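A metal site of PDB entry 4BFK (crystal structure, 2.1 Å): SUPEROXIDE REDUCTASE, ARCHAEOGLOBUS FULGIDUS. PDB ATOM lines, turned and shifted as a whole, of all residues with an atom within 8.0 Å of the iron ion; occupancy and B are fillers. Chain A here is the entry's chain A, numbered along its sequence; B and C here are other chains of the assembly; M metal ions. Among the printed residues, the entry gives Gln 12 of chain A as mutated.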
ATOM      1  N   TRP A   9      -0.716  29.318  17.312  1.00  0.00           N
ATOM      2  CA  TRP A   9      -0.160  29.140  18.653  1.00  0.00           C
ATOM      3  C   TRP A   9       1.276  29.640  18.686  1.00  0.00           C
ATOM      4  O   TRP A   9       1.833  30.028  17.663  1.00  0.00           O
ATOM      5  CB  TRP A   9      -0.199  27.661  19.057  1.00  0.00           C
ATOM      6  CG  TRP A   9      -1.526  27.008  18.813  1.00  0.00           C
ATOM      7  CD1 TRP A   9      -2.760  27.606  18.851  1.00  0.00           C
ATOM      8  CD2 TRP A   9      -1.758  25.637  18.463  1.00  0.00           C
ATOM      9  NE1 TRP A   9      -3.746  26.685  18.548  1.00  0.00           N
ATOM     10  CE2 TRP A   9      -3.154  25.471  18.316  1.00  0.00           C
ATOM     11  CE3 TRP A   9      -0.920  24.530  18.263  1.00  0.00           C
ATOM     12  CZ2 TRP A   9      -3.725  24.248  17.974  1.00  0.00           C
ATOM     13  CZ3 TRP A   9      -1.489  23.328  17.928  1.00  0.00           C
ATOM     14  CH2 TRP A   9      -2.881  23.196  17.790  1.00  0.00           C
ATOM     15  N   GLN A  12       3.419  26.842  16.695  1.00  0.00           N
ATOM     16  CA  GLN A  12       2.859  26.093  15.573  1.00  0.00           C
ATOM     17  C   GLN A  12       1.912  26.969  14.737  1.00  0.00           C
ATOM     18  O   GLN A  12       0.896  27.457  15.226  1.00  0.00           O
ATOM     19  CB  GLN A  12       2.127  24.839  16.064  1.00  0.00           C
ATOM     20  CG  GLN A  12       2.885  24.055  17.109  1.00  0.00           C
ATOM     21  CD  GLN A  12       2.183  22.765  17.469  1.00  0.00           C
ATOM     22  OE1 GLN A  12       1.418  22.228  16.677  1.00  0.00           O
ATOM     23  NE2 GLN A  12       2.430  22.278  18.679  1.00  0.00           N
ATOM     24  N   LYS A  13       2.267  27.157  13.481  1.00  0.00           N
ATOM     25  CA  LYS A  13       1.432  27.941  12.573  1.00  0.00           C
ATOM     26  C   LYS A  13       0.580  27.033  11.676  1.00  0.00           C
ATOM     27  O   LYS A  13       1.081  26.169  10.946  1.00  0.00           O
ATOM     28  CB  LYS A  13       2.249  28.970  11.773  1.00  0.00           C
ATOM     29  CG  LYS A  13       3.240  28.402  10.747  1.00  0.00           C
ATOM     30  CD  LYS A  13       4.412  27.650  11.359  1.00  0.00           C
ATOM     31  CE  LYS A  13       4.204  26.129  11.365  1.00  0.00           C
ATOM     32  NZ  LYS A  13       5.418  25.363  11.797  1.00  0.00           N
ATOM     33  N   HIS A  14      -0.732  27.203  11.791  1.00  0.00           N
ATOM     34  CA  HIS A  14      -1.668  26.433  11.008  1.00  0.00           C
ATOM     35  C   HIS A  14      -2.498  27.316  10.101  1.00  0.00           C
ATOM     36  O   HIS A  14      -3.066  26.841   9.130  1.00  0.00           O
ATOM     37  CB  HIS A  14      -2.603  25.653  11.924  1.00  0.00           C
ATOM     38  CG  HIS A  14      -1.970  24.476  12.606  1.00  0.00           C
ATOM     39  ND1 HIS A  14      -1.411  24.557  13.862  1.00  0.00           N
ATOM     40  CD2 HIS A  14      -1.832  23.189  12.216  1.00  0.00           C
ATOM     41  CE1 HIS A  14      -0.955  23.366  14.216  1.00  0.00           C
ATOM     42  NE2 HIS A  14      -1.185  22.529  13.234  1.00  0.00           N
ATOM     43  N   VAL A  34       0.465  26.789   4.107  1.00  0.00           N
ATOM     44  CA  VAL A  34       0.533  26.642   5.551  1.00  0.00           C
ATOM     45  C   VAL A  34       1.990  26.372   5.901  1.00  0.00           C
ATOM     46  O   VAL A  34       2.593  25.423   5.384  1.00  0.00           O
ATOM     47  CB  VAL A  34      -0.364  25.490   6.076  1.00  0.00           C
ATOM     48  CG1 VAL A  34      -0.121  25.245   7.552  1.00  0.00           C
ATOM     49  CG2 VAL A  34      -1.842  25.789   5.808  1.00  0.00           C
ATOM     50  N   HIS A  40       5.297  23.397   8.889  1.00  0.00           N
ATOM     51  CA  HIS A  40       4.434  22.518   9.667  1.00  0.00           C
ATOM     52  C   HIS A  40       4.883  21.083   9.364  1.00  0.00           C
ATOM     53  O   HIS A  40       5.313  20.798   8.264  1.00  0.00           O
ATOM     54  CB  HIS A  40       2.970  22.720   9.243  1.00  0.00           C
ATOM     55  CG  HIS A  40       2.006  21.808   9.936  1.00  0.00           C
ATOM     56  ND1 HIS A  40       1.799  20.498   9.555  1.00  0.00           N
ATOM     57  CD2 HIS A  40       1.175  22.030  10.983  1.00  0.00           C
ATOM     58  CE1 HIS A  40       0.883  19.955  10.338  1.00  0.00           C
ATOM     59  NE2 HIS A  40       0.484  20.857  11.216  1.00  0.00           N
ATOM     60  N   PRO A  41       4.810  20.184  10.361  1.00  0.00           N
ATOM     61  CA  PRO A  41       5.240  18.801  10.091  1.00  0.00           C
ATOM     62  C   PRO A  41       4.502  18.158   8.900  1.00  0.00           C
ATOM     63  O   PRO A  41       3.357  18.517   8.601  1.00  0.00           O
ATOM     64  CB  PRO A  41       4.876  18.056  11.387  1.00  0.00           C
ATOM     65  CG  PRO A  41       4.948  19.107  12.448  1.00  0.00           C
ATOM     66  CD  PRO A  41       4.451  20.378  11.777  1.00  0.00           C
ATOM     67  N   GLU A  45       1.721  10.600  10.372  1.00  0.00           N
ATOM     68  CA  GLU A  45       1.011  10.792  11.635  1.00  0.00           C
ATOM     69  C   GLU A  45       0.552  12.236  11.886  1.00  0.00           C
ATOM     70  O   GLU A  45      -0.305  12.462  12.748  1.00  0.00           O
ATOM     71  CB  GLU A  45       1.898  10.336  12.799  1.00  0.00           C
ATOM     72  CG  GLU A  45       2.315   8.878  12.699  1.00  0.00           C
ATOM     73  CD  GLU A  45       3.608   8.688  11.904  1.00  0.00           C
ATOM     74  OE1 GLU A  45       4.321   9.679  11.682  1.00  0.00           O
ATOM     75  OE2 GLU A  45       3.908   7.535  11.517  1.00  0.00           O
ATOM     76  N   HIS A  46       1.109  13.187  11.152  1.00  0.00           N
ATOM     77  CA  HIS A  46       0.829  14.607  11.364  1.00  0.00           C
ATOM     78  C   HIS A  46       1.114  15.427  10.104  1.00  0.00           C
ATOM     79  O   HIS A  46       2.278  15.558   9.704  1.00  0.00           O
ATOM     80  CB  HIS A  46       1.659  15.152  12.529  1.00  0.00           C
ATOM     81  CG  HIS A  46       1.319  16.569  12.895  1.00  0.00           C
ATOM     82  ND1 HIS A  46       2.092  17.311  13.755  1.00  0.00           N
ATOM     83  CD2 HIS A  46       0.296  17.371  12.520  1.00  0.00           C
ATOM     84  CE1 HIS A  46       1.565  18.511  13.905  1.00  0.00           C
ATOM     85  NE2 HIS A  46       0.471  18.577  13.154  1.00  0.00           N
ATOM     86  N   HIS A  47       0.066  15.996   9.508  1.00  0.00           N
ATOM     87  CA  HIS A  47       0.186  16.704   8.223  1.00  0.00           C
ATOM     88  C   HIS A  47      -1.033  17.582   7.905  1.00  0.00           C
ATOM     89  O   HIS A  47      -2.121  17.379   8.449  1.00  0.00           O
ATOM     90  CB  HIS A  47       0.375  15.705   7.068  1.00  0.00           C
ATOM     91  CG  HIS A  47      -0.680  14.636   7.017  1.00  0.00           C
ATOM     92  ND1 HIS A  47      -0.458  13.340   7.435  1.00  0.00           N
ATOM     93  CD2 HIS A  47      -1.961  14.669   6.583  1.00  0.00           C
ATOM     94  CE1 HIS A  47      -1.550  12.623   7.264  1.00  0.00           C
ATOM     95  NE2 HIS A  47      -2.489  13.410   6.753  1.00  0.00           N
ATOM     96  N   ILE A  48      -0.834  18.560   7.018  1.00  0.00           N
ATOM     97  CA  ILE A  48      -1.931  19.356   6.478  1.00  0.00           C
ATOM     98  C   ILE A  48      -2.499  18.559   5.304  1.00  0.00           C
ATOM     99  O   ILE A  48      -1.741  18.184   4.416  1.00  0.00           O
ATOM    100  CB  ILE A  48      -1.435  20.723   5.965  1.00  0.00           C
ATOM    101  CG1 ILE A  48      -0.740  21.496   7.098  1.00  0.00           C
ATOM    102  CG2 ILE A  48      -2.570  21.526   5.360  1.00  0.00           C
ATOM    103  CD1 ILE A  48      -1.611  21.596   8.374  1.00  0.00           C
ATOM    104  N   TYR A 109      -6.972  22.055   6.840  1.00  0.00           N
ATOM    105  CA  TYR A 109      -7.230  20.997   7.817  1.00  0.00           C
ATOM    106  C   TYR A 109      -5.945  20.294   8.191  1.00  0.00           C
ATOM    107  O   TYR A 109      -5.204  19.829   7.321  1.00  0.00           O
ATOM    108  CB  TYR A 109      -8.232  19.987   7.251  1.00  0.00           C
ATOM    109  CG  TYR A 109      -8.497  18.796   8.161  1.00  0.00           C
ATOM    110  CD1 TYR A 109      -9.016  18.981   9.438  1.00  0.00           C
ATOM    111  CD2 TYR A 109      -8.235  17.492   7.751  1.00  0.00           C
ATOM    112  CE1 TYR A 109      -9.269  17.876  10.293  1.00  0.00           C
ATOM    113  CE2 TYR A 109      -8.492  16.395   8.584  1.00  0.00           C
ATOM    114  CZ  TYR A 109      -9.007  16.601   9.855  1.00  0.00           C
ATOM    115  OH  TYR A 109      -9.262  15.519  10.688  1.00  0.00           O
ATOM    116  N   CYS A 110      -5.671  20.243   9.494  1.00  0.00           N
ATOM    117  CA  CYS A 110      -4.584  19.435  10.018  1.00  0.00           C
ATOM    118  C   CYS A 110      -5.206  18.150  10.558  1.00  0.00           C
ATOM    119  O   CYS A 110      -6.221  18.203  11.246  1.00  0.00           O
ATOM    120  CB  CYS A 110      -3.873  20.177  11.154  1.00  0.00           C
ATOM    121  SG  CYS A 110      -2.535  19.232  11.933  1.00  0.00           S
ATOM    122  N   ASN A 111      -4.629  17.004  10.244  1.00  0.00           N
ATOM    123  CA  ASN A 111      -5.279  15.749  10.629  1.00  0.00           C
ATOM    124  C   ASN A 111      -5.360  15.528  12.152  1.00  0.00           C
ATOM    125  O   ASN A 111      -6.162  14.715  12.603  1.00  0.00           O
ATOM    126  CB  ASN A 111      -4.640  14.536   9.923  1.00  0.00           C
ATOM    127  CG  ASN A 111      -3.251  14.221  10.441  1.00  0.00           C
ATOM    128  OD1 ASN A 111      -2.507  15.123  10.864  1.00  0.00           O
ATOM    129  ND2 ASN A 111      -2.881  12.939  10.404  1.00  0.00           N
ATOM    130  N   ILE A 112      -4.584  16.272  12.940  1.00  0.00           N
ATOM    131  CA  ILE A 112      -4.667  16.174  14.414  1.00  0.00           C
ATOM    132  C   ILE A 112      -4.980  17.498  15.108  1.00  0.00           C
ATOM    133  O   ILE A 112      -5.337  17.528  16.279  1.00  0.00           O
ATOM    134  CB  ILE A 112      -3.386  15.563  15.047  1.00  0.00           C
ATOM    135  CG1 ILE A 112      -2.205  16.547  14.962  1.00  0.00           C
ATOM    136  CG2 ILE A 112      -3.085  14.195  14.436  1.00  0.00           C
ATOM    137  CD1 ILE A 112      -0.914  16.076  15.655  1.00  0.00           C
ATOM    138  N   HIS A 113      -4.862  18.591  14.358  1.00  0.00           N
ATOM    139  CA  HIS A 113      -5.049  19.915  14.932  1.00  0.00           C
ATOM    140  C   HIS A 113      -6.251  20.676  14.380  1.00  0.00           C
ATOM    141  O   HIS A 113      -6.327  21.898  14.500  1.00  0.00           O
ATOM    142  CB  HIS A 113      -3.769  20.750  14.801  1.00  0.00           C
ATOM    143  CG  HIS A 113      -2.671  20.272  15.702  1.00  0.00           C
ATOM    144  ND1 HIS A 113      -1.358  20.167  15.300  1.00  0.00           N
ATOM    145  CD2 HIS A 113      -2.707  19.851  16.989  1.00  0.00           C
ATOM    146  CE1 HIS A 113      -0.624  19.716  16.299  1.00  0.00           C
ATOM    147  NE2 HIS A 113      -1.425  19.506  17.335  1.00  0.00           N
ATOM    148  N   GLY A 114      -7.185  19.942  13.785  1.00  0.00           N
ATOM    149  CA  GLY A 114      -8.476  20.496  13.430  1.00  0.00           C
ATOM    150  C   GLY A 114      -8.472  21.454  12.248  1.00  0.00           C
ATOM    151  O   GLY A 114      -7.589  21.424  11.406  1.00  0.00           O
ATOM    152  N   TRP A 116      -8.968  25.255  10.177  1.00  0.00           N
ATOM    153  CA  TRP A 116      -8.367  26.582  10.223  1.00  0.00           C
ATOM    154  C   TRP A 116      -8.911  27.488   9.125  1.00  0.00           C
ATOM    155  O   TRP A 116      -9.355  27.012   8.090  1.00  0.00           O
ATOM    156  CB  TRP A 116      -6.845  26.453  10.119  1.00  0.00           C
ATOM    157  CG  TRP A 116      -6.307  25.732  11.288  1.00  0.00           C
ATOM    158  CD1 TRP A 116      -6.299  24.374  11.479  1.00  0.00           C
ATOM    159  CD2 TRP A 116      -5.766  26.297  12.478  1.00  0.00           C
ATOM    160  NE1 TRP A 116      -5.759  24.074  12.701  1.00  0.00           N
ATOM    161  CE2 TRP A 116      -5.428  25.242  13.350  1.00  0.00           C
ATOM    162  CE3 TRP A 116      -5.524  27.621  12.903  1.00  0.00           C
ATOM    163  CZ2 TRP A 116      -4.863  25.437  14.608  1.00  0.00           C
ATOM    164  CZ3 TRP A 116      -4.947  27.821  14.155  1.00  0.00           C
ATOM    165  CH2 TRP A 116      -4.615  26.741  14.983  1.00  0.00           C
ATOM    166  N   VAL B  78      -3.406  14.111  18.677  1.00  0.00           N
ATOM    167  CA  VAL B  78      -2.287  14.714  19.392  1.00  0.00           C
ATOM    168  C   VAL B  78      -1.664  13.729  20.390  1.00  0.00           C
ATOM    169  O   VAL B  78      -0.548  13.941  20.859  1.00  0.00           O
ATOM    170  CB  VAL B  78      -2.699  16.030  20.119  1.00  0.00           C
ATOM    171  CG1 VAL B  78      -3.027  17.116  19.105  1.00  0.00           C
ATOM    172  CG2 VAL B  78      -3.876  15.792  21.056  1.00  0.00           C
ATOM    173  N   PHE C  62      -9.761  18.637  19.441  1.00  0.00           N
ATOM    174  CA  PHE C  62      -9.936  18.921  18.014  1.00  0.00           C
ATOM    175  C   PHE C  62     -10.968  18.025  17.321  1.00  0.00           C
ATOM    176  O   PHE C  62     -11.127  16.837  17.660  1.00  0.00           O
ATOM    177  CB  PHE C  62      -8.588  18.856  17.295  1.00  0.00           C
ATOM    178  CG  PHE C  62      -7.537  19.723  17.919  1.00  0.00           C
ATOM    179  CD1 PHE C  62      -7.501  21.090  17.665  1.00  0.00           C
ATOM    180  CD2 PHE C  62      -6.597  19.182  18.791  1.00  0.00           C
ATOM    181  CE1 PHE C  62      -6.535  21.898  18.259  1.00  0.00           C
ATOM    182  CE2 PHE C  62      -5.621  19.982  19.379  1.00  0.00           C
ATOM    183  CZ  PHE C  62      -5.595  21.344  19.116  1.00  0.00           C
HETATM  184 FE    FE M   1      -0.766  20.364  13.110  1.00  0.00          FE
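The indole nitrogen (NE1) of Trp 116 lies within hydrogen-bond range of the backbone carbonyl oxygen (O) of His 113. SG of Cys 110 sits close to N of Ile 112, at 3.7 Å.
Within 4 Å of the iron ion: His 14, His 40, His 46, Cys 110 and His 113. The nearest printed residue that does not touch the iron ion is Ile 112 (4.5 Å).
The iron ion is bound by NE2 of His 46 (2.2 Å), NE2 of His 14 (2.2 Å), ND1 of His 113 (2.3 Å), NE2 of His 40 (2.3 Å) and SG of Cys 110 (2.4 Å). The iron ion has five donor atoms within binding distance.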
